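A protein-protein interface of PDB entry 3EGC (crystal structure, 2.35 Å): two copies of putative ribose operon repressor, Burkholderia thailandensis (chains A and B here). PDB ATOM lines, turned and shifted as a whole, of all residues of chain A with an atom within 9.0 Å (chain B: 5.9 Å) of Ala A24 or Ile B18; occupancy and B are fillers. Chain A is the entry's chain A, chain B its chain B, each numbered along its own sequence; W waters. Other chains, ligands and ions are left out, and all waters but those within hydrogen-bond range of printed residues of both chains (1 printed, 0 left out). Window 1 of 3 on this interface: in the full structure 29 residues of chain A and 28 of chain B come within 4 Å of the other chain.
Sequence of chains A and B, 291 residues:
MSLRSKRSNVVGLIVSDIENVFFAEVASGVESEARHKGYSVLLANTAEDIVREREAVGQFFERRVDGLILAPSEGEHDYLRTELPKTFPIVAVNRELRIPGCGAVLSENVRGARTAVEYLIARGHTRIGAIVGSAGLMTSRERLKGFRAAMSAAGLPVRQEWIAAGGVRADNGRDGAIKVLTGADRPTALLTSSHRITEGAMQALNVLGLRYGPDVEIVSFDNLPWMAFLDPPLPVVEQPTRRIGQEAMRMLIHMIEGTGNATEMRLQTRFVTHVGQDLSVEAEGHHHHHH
OG of Ser A28 sits at hydrogen-bond distance from OE2 of Glu B19. OG of Ser A28 lies within hydrogen-bond range of ND2 of Asn B45, at 3.4 Å. OE1 of Glu A31 sits close to N of Asn B45 (3.2 Å). NH1 of Arg A242 lies within salt-bridge range of OE1 of Glu B19 (2.4 Å).
The side-chain carboxylate (OD1) of Asp A17 lies within hydrogen-bond range of the backbone NH (N) of Glu A19 (3.1 Å). The backbone NH (N) of Ile A18 is in hydrogen-bond range of the side-chain amide oxygen (OD1) of Asn A45, at 2.9 Å. The side-chain hydroxyl of Thr A241 sits at hydrogen-bond distance from the side-chain carboxylate of Glu A25, at 2.4 Å. NH2 of Arg A242 lies within salt-bridge range of OE1 of Glu A25 (3.998 Å). The side-chain carboxylate (OD1) of Asp B17 is in hydrogen-bond range of the backbone NH (N) of Glu B19 (3.1 Å). The backbone NH of Ile B18 lies within hydrogen-bond range of the side-chain amide oxygen of Asn B45 (2.8 Å).
Among the printed residues, merely in contact across the chains: Ala A24 with Ile B18 (3.2 Å), Val A21 with Val B21 (3.3 Å), Ile A18 with Ala B24 (3.3 Å), Val A21 with Glu B19 (3.6 Å), Glu A19 with Val B21 (3.6 Å), Glu A31 with Leu B43 (3.7 Å), Ser A28 with Ile B18 (3.8 Å) and Glu A25 with Glu B19 (3.9 Å).
Phe A22 touches none of the printed residues of chain B. Of the printed residues of chain B, Ala A24 touches Ile B18. Of the printed residues of chain B, Glu A25 touches Glu B19 (3.9 Å). Of the printed residues of chain B, Arg A242 touches Glu B19. Printed residues of chain A within 4 Å of Glu B19: Val A21, Glu A25, Ser A28 and Arg A242. Of the printed residues of chain A, Val B21 touches Glu A19 and Val A21. Printed residues of chain A within 4 Å of Asn B45: Ser A28 and Glu A31. The nearest printed residue of chain B that does not touch Ala A24 is Ala B24 (4.001 Å).
Hydrophobic or aromatic side chains of chain B within 4 Å of the printed part of chain A: Ile B18, Val B21 and Ala B24.
Ile A18 touches Ala B24, and with the chains exchanged Ala A24 touches Ile B18. Glu A19 touches Val B21, and with the chains exchanged Val A21 touches Glu B19. Val A21 touches its own counterpart, Val B21. Positions printed for both chains: 13, 15, 16, 17, 18, 19, 20, 21, 23, 24, 27, 43 and 45. Of the 12 pairs that touch across the chains among the printed residues, 5 have their exchanged pair printed and touching as well.
Water W1 lies within hydrogen-bond range of the backbone carbonyl oxygen of Ser A28 (2.6 Å), the side-chain carboxylate of Glu A31 (2.9 Å) and the side-chain amide nitrogen of Asn B45 (3.0 Å).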
ATOM      1  N   LEU A  13      14.821  -9.341  -8.789  1.00  0.00           N
ATOM      2  CA  LEU A  13      13.424  -9.236  -8.380  1.00  0.00           C
ATOM      3  C   LEU A  13      12.685 -10.447  -8.918  1.00  0.00           C
ATOM      4  O   LEU A  13      12.712 -10.726 -10.124  1.00  0.00           O
ATOM      5  CB  LEU A  13      12.754  -7.970  -8.874  1.00  0.00           C
ATOM      6  CG  LEU A  13      11.235  -7.880  -8.712  1.00  0.00           C
ATOM      7  CD1 LEU A  13      10.780  -7.952  -7.224  1.00  0.00           C
ATOM      8  CD2 LEU A  13      10.635  -6.620  -9.370  1.00  0.00           C
ATOM      9  N   VAL A  15       9.146 -12.439  -8.812  1.00  0.00           N
ATOM     10  CA  VAL A  15       7.785 -12.159  -8.510  1.00  0.00           C
ATOM     11  C   VAL A  15       6.917 -13.376  -8.844  1.00  0.00           C
ATOM     12  O   VAL A  15       7.080 -13.978  -9.898  1.00  0.00           O
ATOM     13  CB  VAL A  15       7.394 -10.888  -9.307  1.00  0.00           C
ATOM     14  CG1 VAL A  15       5.978 -10.909  -9.801  1.00  0.00           C
ATOM     15  CG2 VAL A  15       7.720  -9.634  -8.471  1.00  0.00           C
ATOM     16  N   SER A  16       5.944 -13.694  -7.989  1.00  0.00           N
ATOM     17  CA  SER A  16       5.091 -14.832  -8.214  1.00  0.00           C
ATOM     18  C   SER A  16       4.063 -14.662  -9.379  1.00  0.00           C
ATOM     19  O   SER A  16       3.641 -15.687 -10.018  1.00  0.00           O
ATOM     20  CB  SER A  16       4.381 -15.180  -6.941  1.00  0.00           C
ATOM     21  OG  SER A  16       3.828 -14.011  -6.324  1.00  0.00           O
ATOM     22  N   ASP A  17       3.667 -13.414  -9.679  1.00  0.00           N
ATOM     23  CA  ASP A  17       2.803 -13.212 -10.821  1.00  0.00           C
ATOM     24  C   ASP A  17       2.787 -11.780 -11.397  1.00  0.00           C
ATOM     25  O   ASP A  17       1.931 -10.991 -11.038  1.00  0.00           O
ATOM     26  CB  ASP A  17       1.373 -13.685 -10.511  1.00  0.00           C
ATOM     27  CG  ASP A  17       0.480 -13.607 -11.701  1.00  0.00           C
ATOM     28  OD1 ASP A  17       0.968 -13.280 -12.822  1.00  0.00           O
ATOM     29  OD2 ASP A  17      -0.731 -13.841 -11.533  1.00  0.00           O
ATOM     30  N   ILE A  18       3.737 -11.475 -12.289  1.00  0.00           N
ATOM     31  CA  ILE A  18       3.862 -10.109 -12.810  1.00  0.00           C
ATOM     32  C   ILE A  18       2.549  -9.593 -13.544  1.00  0.00           C
ATOM     33  O   ILE A  18       2.269  -8.383 -13.596  1.00  0.00           O
ATOM     34  CB  ILE A  18       5.105  -9.974 -13.707  1.00  0.00           C
ATOM     35  CG1 ILE A  18       5.459  -8.490 -13.919  1.00  0.00           C
ATOM     36  CG2 ILE A  18       4.878 -10.711 -15.067  1.00  0.00           C
ATOM     37  CD1 ILE A  18       5.897  -7.831 -12.643  1.00  0.00           C
ATOM     38  N   GLU A  19       1.734 -10.528 -14.059  1.00  0.00           N
ATOM     39  CA  GLU A  19       0.510 -10.174 -14.811  1.00  0.00           C
ATOM     40  C   GLU A  19      -0.607  -9.665 -13.871  1.00  0.00           C
ATOM     41  O   GLU A  19      -1.588  -9.081 -14.308  1.00  0.00           O
ATOM     42  CB  GLU A  19       0.018 -11.371 -15.610  1.00  0.00           C
ATOM     43  CG  GLU A  19       1.038 -11.958 -16.623  1.00  0.00           C
ATOM     44  CD  GLU A  19       0.556 -13.292 -17.208  1.00  0.00           C
ATOM     45  OE1 GLU A  19      -0.594 -13.669 -16.871  1.00  0.00           O
ATOM     46  OE2 GLU A  19       1.307 -13.982 -17.965  1.00  0.00           O
ATOM     47  N   ASN A  20      -0.444  -9.939 -12.575  1.00  0.00           N
ATOM     48  CA  ASN A  20      -1.342  -9.475 -11.534  1.00  0.00           C
ATOM     49  C   ASN A  20      -0.824  -8.059 -11.177  1.00  0.00           C
ATOM     50  O   ASN A  20       0.366  -7.809 -10.919  1.00  0.00           O
ATOM     51  CB  ASN A  20      -1.317 -10.427 -10.352  1.00  0.00           C
ATOM     52  CG  ASN A  20      -2.229  -9.967  -9.154  1.00  0.00           C
ATOM     53  OD1 ASN A  20      -2.535  -8.826  -9.007  1.00  0.00           O
ATOM     54  ND2 ASN A  20      -2.668 -10.930  -8.333  1.00  0.00           N
ATOM     55  N   VAL A  21      -1.756  -7.147 -11.233  1.00  0.00           N
ATOM     56  CA  VAL A  21      -1.499  -5.757 -11.133  1.00  0.00           C
ATOM     57  C   VAL A  21      -0.873  -5.421  -9.776  1.00  0.00           C
ATOM     58  O   VAL A  21      -0.109  -4.464  -9.670  1.00  0.00           O
ATOM     59  CB  VAL A  21      -2.841  -4.990 -11.404  1.00  0.00           C
ATOM     60  CG1 VAL A  21      -3.125  -4.024 -10.313  1.00  0.00           C
ATOM     61  CG2 VAL A  21      -2.745  -4.256 -12.656  1.00  0.00           C
ATOM     62  N   PHE A  22      -1.185  -6.216  -8.759  1.00  0.00           N
ATOM     63  CA  PHE A  22      -0.564  -6.038  -7.476  1.00  0.00           C
ATOM     64  C   PHE A  22       0.971  -6.028  -7.592  1.00  0.00           C
ATOM     65  O   PHE A  22       1.635  -5.096  -7.162  1.00  0.00           O
ATOM     66  CB  PHE A  22      -1.045  -7.115  -6.495  1.00  0.00           C
ATOM     67  CG  PHE A  22      -0.364  -7.046  -5.156  1.00  0.00           C
ATOM     68  CD1 PHE A  22      -0.847  -6.251  -4.143  1.00  0.00           C
ATOM     69  CD2 PHE A  22       0.796  -7.793  -4.917  1.00  0.00           C
ATOM     70  CE1 PHE A  22      -0.157  -6.205  -2.894  1.00  0.00           C
ATOM     71  CE2 PHE A  22       1.448  -7.765  -3.723  1.00  0.00           C
ATOM     72  CZ  PHE A  22       0.972  -6.987  -2.710  1.00  0.00           C
ATOM     73  N   PHE A  23       1.506  -7.113  -8.149  1.00  0.00           N
ATOM     74  CA  PHE A  23       2.927  -7.348  -8.333  1.00  0.00           C
ATOM     75  C   PHE A  23       3.628  -6.402  -9.339  1.00  0.00           C
ATOM     76  O   PHE A  23       4.771  -6.092  -9.185  1.00  0.00           O
ATOM     77  CB  PHE A  23       3.169  -8.853  -8.712  1.00  0.00           C
ATOM     78  CG  PHE A  23       2.774  -9.807  -7.628  1.00  0.00           C
ATOM     79  CD1 PHE A  23       3.468  -9.840  -6.400  1.00  0.00           C
ATOM     80  CD2 PHE A  23       1.684 -10.649  -7.802  1.00  0.00           C
ATOM     81  CE1 PHE A  23       3.052 -10.673  -5.377  1.00  0.00           C
ATOM     82  CE2 PHE A  23       1.273 -11.525  -6.781  1.00  0.00           C
ATOM     83  CZ  PHE A  23       1.947 -11.528  -5.548  1.00  0.00           C
ATOM     84  N   ALA A  24       2.941  -6.028 -10.400  1.00  0.00           N
ATOM     85  CA  ALA A  24       3.388  -4.999 -11.307  1.00  0.00           C
ATOM     86  C   ALA A  24       3.614  -3.629 -10.621  1.00  0.00           C
ATOM     87  O   ALA A  24       4.568  -2.896 -10.944  1.00  0.00           O
ATOM     88  CB  ALA A  24       2.350  -4.814 -12.511  1.00  0.00           C
ATOM     89  N   GLU A  25       2.682  -3.254  -9.767  1.00  0.00           N
ATOM     90  CA  GLU A  25       2.846  -2.002  -9.000  1.00  0.00           C
ATOM     91  C   GLU A  25       3.960  -2.120  -7.904  1.00  0.00           C
ATOM     92  O   GLU A  25       4.636  -1.152  -7.626  1.00  0.00           O
ATOM     93  CB  GLU A  25       1.528  -1.590  -8.354  1.00  0.00           C
ATOM     94  CG  GLU A  25       0.396  -1.168  -9.313  1.00  0.00           C
ATOM     95  CD  GLU A  25      -0.911  -0.872  -8.534  1.00  0.00           C
ATOM     96  OE1 GLU A  25      -0.970  -0.961  -7.277  1.00  0.00           O
ATOM     97  OE2 GLU A  25      -1.903  -0.479  -9.139  1.00  0.00           O
ATOM     98  N   VAL A  26       4.135  -3.302  -7.302  1.00  0.00           N
ATOM     99  CA  VAL A  26       5.276  -3.515  -6.367  1.00  0.00           C
ATOM    100  C   VAL A  26       6.625  -3.426  -7.124  1.00  0.00           C
ATOM    101  O   VAL A  26       7.589  -2.826  -6.642  1.00  0.00           O
ATOM    102  CB  VAL A  26       5.229  -4.926  -5.681  1.00  0.00           C
ATOM    103  CG1 VAL A  26       6.567  -5.232  -4.996  1.00  0.00           C
ATOM    104  CG2 VAL A  26       3.999  -5.026  -4.640  1.00  0.00           C
ATOM    105  N   ALA A  27       6.660  -4.042  -8.322  1.00  0.00           N
ATOM    106  CA  ALA A  27       7.836  -4.028  -9.160  1.00  0.00           C
ATOM    107  C   ALA A  27       8.219  -2.579  -9.547  1.00  0.00           C
ATOM    108  O   ALA A  27       9.432  -2.234  -9.563  1.00  0.00           O
ATOM    109  CB  ALA A  27       7.575  -4.851 -10.444  1.00  0.00           C
ATOM    110  N   SER A  28       7.196  -1.796  -9.901  1.00  0.00           N
ATOM    111  CA  SER A  28       7.332  -0.352 -10.199  1.00  0.00           C
ATOM    112  C   SER A  28       8.025   0.385  -9.012  1.00  0.00           C
ATOM    113  O   SER A  28       9.002   1.067  -9.203  1.00  0.00           O
ATOM    114  CB  SER A  28       5.932   0.248 -10.443  1.00  0.00           C
ATOM    115  OG  SER A  28       6.044   1.588 -10.610  1.00  0.00           O
ATOM    116  N   GLY A  29       7.537   0.187  -7.796  1.00  0.00           N
ATOM    117  CA  GLY A  29       8.161   0.786  -6.588  1.00  0.00           C
ATOM    118  C   GLY A  29       9.610   0.340  -6.366  1.00  0.00           C
ATOM    119  O   GLY A  29      10.512   1.182  -5.993  1.00  0.00           O
ATOM    120  N   VAL A  30       9.852  -0.967  -6.568  1.00  0.00           N
ATOM    121  CA  VAL A  30      11.201  -1.516  -6.472  1.00  0.00           C
ATOM    122  C   VAL A  30      12.179  -0.870  -7.536  1.00  0.00           C
ATOM    123  O   VAL A  30      13.281  -0.443  -7.211  1.00  0.00           O
ATOM    124  CB  VAL A  30      11.209  -3.017  -6.773  1.00  0.00           C
ATOM    125  CG1 VAL A  30      12.620  -3.461  -6.994  1.00  0.00           C
ATOM    126  CG2 VAL A  30      10.513  -3.814  -5.718  1.00  0.00           C
ATOM    127  N   GLU A  31      11.725  -0.793  -8.782  1.00  0.00           N
ATOM    128  CA  GLU A  31      12.530  -0.276  -9.869  1.00  0.00           C
ATOM    129  C   GLU A  31      12.836   1.208  -9.712  1.00  0.00           C
ATOM    130  O   GLU A  31      13.909   1.655 -10.013  1.00  0.00           O
ATOM    131  CB  GLU A  31      11.832  -0.521 -11.229  1.00  0.00           C
ATOM    132  CG  GLU A  31      12.716  -0.263 -12.428  1.00  0.00           C
ATOM    133  CD  GLU A  31      12.629   1.178 -12.916  1.00  0.00           C
ATOM    134  OE1 GLU A  31      13.519   1.526 -13.674  1.00  0.00           O
ATOM    135  OE2 GLU A  31      11.710   1.943 -12.551  1.00  0.00           O
ATOM    136  N   SER A  32      11.872   1.957  -9.209  1.00  0.00           N
ATOM    137  CA  SER A  32      12.024   3.378  -9.002  1.00  0.00           C
ATOM    138  C   SER A  32      13.032   3.651  -7.860  1.00  0.00           C
ATOM    139  O   SER A  32      13.904   4.520  -7.944  1.00  0.00           O
ATOM    140  CB  SER A  32      10.644   3.920  -8.645  1.00  0.00           C
ATOM    141  OG  SER A  32      10.618   5.316  -8.651  1.00  0.00           O
ATOM    142  N   LEU A  43      14.694  -9.213 -13.753  1.00  0.00           N
ATOM    143  CA  LEU A  43      13.330  -9.632 -13.441  1.00  0.00           C
ATOM    144  C   LEU A  43      13.092 -11.093 -13.744  1.00  0.00           C
ATOM    145  O   LEU A  43      13.530 -11.585 -14.759  1.00  0.00           O
ATOM    146  CB  LEU A  43      12.312  -8.774 -14.158  1.00  0.00           C
ATOM    147  CG  LEU A  43      10.875  -9.262 -14.184  1.00  0.00           C
ATOM    148  CD1 LEU A  43      10.199  -9.039 -12.800  1.00  0.00           C
ATOM    149  CD2 LEU A  43      10.074  -8.531 -15.349  1.00  0.00           C
ATOM    150  N   ASN A  45       9.774 -13.937 -13.499  1.00  0.00           N
ATOM    151  CA  ASN A  45       8.351 -14.179 -13.223  1.00  0.00           C
ATOM    152  C   ASN A  45       8.115 -15.655 -13.091  1.00  0.00           C
ATOM    153  O   ASN A  45       8.419 -16.344 -14.000  1.00  0.00           O
ATOM    154  CB  ASN A  45       7.453 -13.618 -14.345  1.00  0.00           C
ATOM    155  CG  ASN A  45       5.961 -13.887 -14.084  1.00  0.00           C
ATOM    156  OD1 ASN A  45       5.455 -13.658 -12.988  1.00  0.00           O
ATOM    157  ND2 ASN A  45       5.275 -14.365 -15.083  1.00  0.00           N
ATOM    158  N   ALA A  71       8.887 -12.058  -4.085  1.00  0.00           N
ATOM    159  CA  ALA A  71       7.472 -12.326  -3.805  1.00  0.00           C
ATOM    160  C   ALA A  71       7.244 -13.849  -3.885  1.00  0.00           C
ATOM    161  O   ALA A  71       7.105 -14.423  -4.975  1.00  0.00           O
ATOM    162  CB  ALA A  71       6.563 -11.605  -4.805  1.00  0.00           C
ATOM    163  N   HIS A 195      -8.456  -8.633  -5.575  1.00  0.00           N
ATOM    164  CA  HIS A 195      -9.217  -8.253  -6.777  1.00  0.00           C
ATOM    165  C   HIS A 195      -9.485  -9.444  -7.668  1.00  0.00           C
ATOM    166  O   HIS A 195     -10.533  -9.532  -8.270  1.00  0.00           O
ATOM    167  CB  HIS A 195      -8.536  -7.127  -7.558  1.00  0.00           C
ATOM    168  CG  HIS A 195      -7.244  -7.517  -8.216  1.00  0.00           C
ATOM    169  ND1 HIS A 195      -7.138  -7.714  -9.576  1.00  0.00           N
ATOM    170  CD2 HIS A 195      -5.994  -7.686  -7.714  1.00  0.00           C
ATOM    171  CE1 HIS A 195      -5.877  -8.003  -9.884  1.00  0.00           C
ATOM    172  NE2 HIS A 195      -5.161  -8.002  -8.769  1.00  0.00           N
ATOM    173  N   THR A 241       0.875  -0.599  -2.567  1.00  0.00           N
ATOM    174  CA  THR A 241       1.714  -1.468  -3.435  1.00  0.00           C
ATOM    175  C   THR A 241       3.038  -0.898  -3.829  1.00  0.00           C
ATOM    176  O   THR A 241       4.057  -1.565  -3.709  1.00  0.00           O
ATOM    177  CB  THR A 241       0.986  -1.832  -4.745  1.00  0.00           C
ATOM    178  OG1 THR A 241       0.519  -0.615  -5.403  1.00  0.00           O
ATOM    179  CG2 THR A 241      -0.182  -2.685  -4.459  1.00  0.00           C
ATOM    180  N   ARG A 242       3.037   0.333  -4.298  1.00  0.00           N
ATOM    181  CA  ARG A 242       4.286   1.001  -4.633  1.00  0.00           C
ATOM    182  C   ARG A 242       5.259   1.159  -3.472  1.00  0.00           C
ATOM    183  O   ARG A 242       6.443   0.914  -3.618  1.00  0.00           O
ATOM    184  CB  ARG A 242       3.991   2.365  -5.323  1.00  0.00           C
ATOM    185  CG  ARG A 242       3.827   2.188  -6.839  1.00  0.00           C
ATOM    186  CD  ARG A 242       2.976   3.341  -7.482  1.00  0.00           C
ATOM    187  NE  ARG A 242       1.582   3.264  -7.049  1.00  0.00           N
ATOM    188  CZ  ARG A 242       0.527   3.097  -7.854  1.00  0.00           C
ATOM    189  NH1 ARG A 242       0.677   3.038  -9.177  1.00  0.00           N
ATOM    190  NH2 ARG A 242      -0.700   3.028  -7.312  1.00  0.00           N
ATOM    191  N   GLY A 245       7.055  -2.065  -2.613  1.00  0.00           N
ATOM    192  CA  GLY A 245       8.260  -2.215  -3.464  1.00  0.00           C
ATOM    193  C   GLY A 245       9.435  -1.281  -3.109  1.00  0.00           C
ATOM    194  O   GLY A 245      10.597  -1.714  -3.039  1.00  0.00           O
ATOM    195  N   LEU B  13      14.718  -4.611 -20.936  1.00  0.00           N
ATOM    196  CA  LEU B  13      13.318  -4.402 -21.251  1.00  0.00           C
ATOM    197  C   LEU B  13      12.945  -3.094 -20.598  1.00  0.00           C
ATOM    198  O   LEU B  13      13.038  -2.957 -19.373  1.00  0.00           O
ATOM    199  CB  LEU B  13      12.441  -5.517 -20.692  1.00  0.00           C
ATOM    200  CG  LEU B  13      10.925  -5.325 -20.760  1.00  0.00           C
ATOM    201  CD1 LEU B  13      10.424  -5.218 -22.186  1.00  0.00           C
ATOM    202  CD2 LEU B  13      10.229  -6.481 -19.986  1.00  0.00           C
ATOM    203  N   VAL B  15       9.850  -0.319 -20.413  1.00  0.00           N
ATOM    204  CA  VAL B  15       8.428  -0.308 -20.576  1.00  0.00           C
ATOM    205  C   VAL B  15       7.938   1.086 -20.153  1.00  0.00           C
ATOM    206  O   VAL B  15       8.447   1.706 -19.231  1.00  0.00           O
ATOM    207  CB  VAL B  15       7.793  -1.501 -19.766  1.00  0.00           C
ATOM    208  CG1 VAL B  15       6.436  -1.245 -19.334  1.00  0.00           C
ATOM    209  CG2 VAL B  15       7.804  -2.785 -20.571  1.00  0.00           C
ATOM    210  N   SER B  16       6.983   1.600 -20.875  1.00  0.00           N
ATOM    211  CA  SER B  16       6.462   2.907 -20.565  1.00  0.00           C
ATOM    212  C   SER B  16       5.551   2.879 -19.344  1.00  0.00           C
ATOM    213  O   SER B  16       5.471   3.886 -18.624  1.00  0.00           O
ATOM    214  CB  SER B  16       5.752   3.524 -21.778  1.00  0.00           C
ATOM    215  OG  SER B  16       4.887   2.550 -22.369  1.00  0.00           O
ATOM    216  N   ASP B  17       4.861   1.768 -19.086  1.00  0.00           N
ATOM    217  CA  ASP B  17       4.094   1.735 -17.828  1.00  0.00           C
ATOM    218  C   ASP B  17       3.826   0.336 -17.291  1.00  0.00           C
ATOM    219  O   ASP B  17       2.829  -0.248 -17.647  1.00  0.00           O
ATOM    220  CB  ASP B  17       2.795   2.554 -17.968  1.00  0.00           C
ATOM    221  CG  ASP B  17       1.971   2.578 -16.673  1.00  0.00           C
ATOM    222  OD1 ASP B  17       2.462   2.077 -15.602  1.00  0.00           O
ATOM    223  OD2 ASP B  17       0.819   3.084 -16.725  1.00  0.00           O
ATOM    224  N   ILE B  18       4.712  -0.193 -16.442  1.00  0.00           N
ATOM    225  CA  ILE B  18       4.592  -1.601 -15.964  1.00  0.00           C
ATOM    226  C   ILE B  18       3.299  -1.833 -15.146  1.00  0.00           C
ATOM    227  O   ILE B  18       2.809  -2.938 -15.103  1.00  0.00           O
ATOM    228  CB  ILE B  18       5.874  -2.081 -15.161  1.00  0.00           C
ATOM    229  CG1 ILE B  18       5.881  -3.597 -14.989  1.00  0.00           C
ATOM    230  CG2 ILE B  18       5.974  -1.428 -13.814  1.00  0.00           C
ATOM    231  CD1 ILE B  18       6.263  -4.400 -16.265  1.00  0.00           C
ATOM    232  N   GLU B  19       2.749  -0.782 -14.551  1.00  0.00           N
ATOM    233  CA  GLU B  19       1.576  -0.865 -13.680  1.00  0.00           C
ATOM    234  C   GLU B  19       0.290  -1.094 -14.520  1.00  0.00           C
ATOM    235  O   GLU B  19      -0.719  -1.596 -14.010  1.00  0.00           O
ATOM    236  CB  GLU B  19       1.442   0.430 -12.851  1.00  0.00           C
ATOM    237  CG  GLU B  19       2.630   0.718 -11.914  1.00  0.00           C
ATOM    238  CD  GLU B  19       2.525   2.113 -11.224  1.00  0.00           C
ATOM    239  OE1 GLU B  19       1.517   2.867 -11.445  1.00  0.00           O
ATOM    240  OE2 GLU B  19       3.445   2.473 -10.449  1.00  0.00           O
ATOM    241  N   ASN B  20       0.365  -0.730 -15.803  1.00  0.00           N
ATOM    242  CA  ASN B  20      -0.705  -0.974 -16.755  1.00  0.00           C
ATOM    243  C   ASN B  20      -0.553  -2.412 -17.149  1.00  0.00           C
ATOM    244  O   ASN B  20       0.577  -2.847 -17.525  1.00  0.00           O
ATOM    245  CB  ASN B  20      -0.570  -0.053 -17.979  1.00  0.00           C
ATOM    246  CG  ASN B  20      -1.658  -0.255 -19.017  1.00  0.00           C
ATOM    247  OD1 ASN B  20      -2.178  -1.346 -19.208  1.00  0.00           O
ATOM    248  ND2 ASN B  20      -2.005   0.821 -19.719  1.00  0.00           N
ATOM    249  N   VAL B  21      -1.648  -3.141 -17.034  1.00  0.00           N
ATOM    250  CA  VAL B  21      -1.638  -4.594 -17.161  1.00  0.00           C
ATOM    251  C   VAL B  21      -1.265  -5.081 -18.607  1.00  0.00           C
ATOM    252  O   VAL B  21      -0.872  -6.212 -18.806  1.00  0.00           O
ATOM    253  CB  VAL B  21      -2.985  -5.112 -16.717  1.00  0.00           C
ATOM    254  CG1 VAL B  21      -3.646  -5.983 -17.758  1.00  0.00           C
ATOM    255  CG2 VAL B  21      -2.823  -5.870 -15.512  1.00  0.00           C
ATOM    256  N   PHE B  23       1.182  -3.845 -20.461  1.00  0.00           N
ATOM    257  CA  PHE B  23       2.634  -3.952 -20.414  1.00  0.00           C
ATOM    258  C   PHE B  23       3.141  -5.050 -19.525  1.00  0.00           C
ATOM    259  O   PHE B  23       4.123  -5.704 -19.894  1.00  0.00           O
ATOM    260  CB  PHE B  23       3.262  -2.593 -20.064  1.00  0.00           C
ATOM    261  CG  PHE B  23       2.934  -1.527 -21.071  1.00  0.00           C
ATOM    262  CD1 PHE B  23       3.429  -1.612 -22.360  1.00  0.00           C
ATOM    263  CD2 PHE B  23       2.106  -0.482 -20.756  1.00  0.00           C
ATOM    264  CE1 PHE B  23       3.162  -0.629 -23.320  1.00  0.00           C
ATOM    265  CE2 PHE B  23       1.809   0.518 -21.736  1.00  0.00           C
ATOM    266  CZ  PHE B  23       2.336   0.419 -23.017  1.00  0.00           C
ATOM    267  N   ALA B  24       2.453  -5.279 -18.412  1.00  0.00           N
ATOM    268  CA  ALA B  24       2.847  -6.328 -17.515  1.00  0.00           C
ATOM    269  C   ALA B  24       2.759  -7.689 -18.241  1.00  0.00           C
ATOM    270  O   ALA B  24       3.595  -8.487 -18.108  1.00  0.00           O
ATOM    271  CB  ALA B  24       2.013  -6.310 -16.206  1.00  0.00           C
ATOM    272  N   ALA B  27       5.483  -8.150 -20.753  1.00  0.00           N
ATOM    273  CA  ALA B  27       6.708  -8.385 -20.034  1.00  0.00           C
ATOM    274  C   ALA B  27       6.795  -9.854 -19.621  1.00  0.00           C
ATOM    275  O   ALA B  27       7.836 -10.516 -19.739  1.00  0.00           O
ATOM    276  CB  ALA B  27       6.725  -7.489 -18.861  1.00  0.00           C
ATOM    277  N   LEU B  43      15.003  -4.916 -16.016  1.00  0.00           N
ATOM    278  CA  LEU B  43      13.749  -4.188 -16.167  1.00  0.00           C
ATOM    279  C   LEU B  43      13.883  -2.699 -15.845  1.00  0.00           C
ATOM    280  O   LEU B  43      14.498  -2.340 -14.884  1.00  0.00           O
ATOM    281  CB  LEU B  43      12.658  -4.822 -15.289  1.00  0.00           C
ATOM    282  CG  LEU B  43      11.349  -4.008 -15.154  1.00  0.00           C
ATOM    283  CD1 LEU B  43      10.503  -4.076 -16.456  1.00  0.00           C
ATOM    284  CD2 LEU B  43      10.553  -4.530 -13.929  1.00  0.00           C
ATOM    285  N   ASN B  45      11.176   0.741 -15.714  1.00  0.00           N
ATOM    286  CA  ASN B  45       9.846   1.348 -15.909  1.00  0.00           C
ATOM    287  C   ASN B  45       9.987   2.892 -16.044  1.00  0.00           C
ATOM    288  O   ASN B  45      10.616   3.495 -15.223  1.00  0.00           O
ATOM    289  CB  ASN B  45       8.933   0.977 -14.704  1.00  0.00           C
ATOM    290  CG  ASN B  45       7.545   1.573 -14.814  1.00  0.00           C
ATOM    291  OD1 ASN B  45       6.879   1.403 -15.858  1.00  0.00           O
ATOM    292  ND2 ASN B  45       7.087   2.261 -13.756  1.00  0.00           N
HETATM  293  O   HOH W   1       9.065   2.188 -11.501  1.00  0.00           O
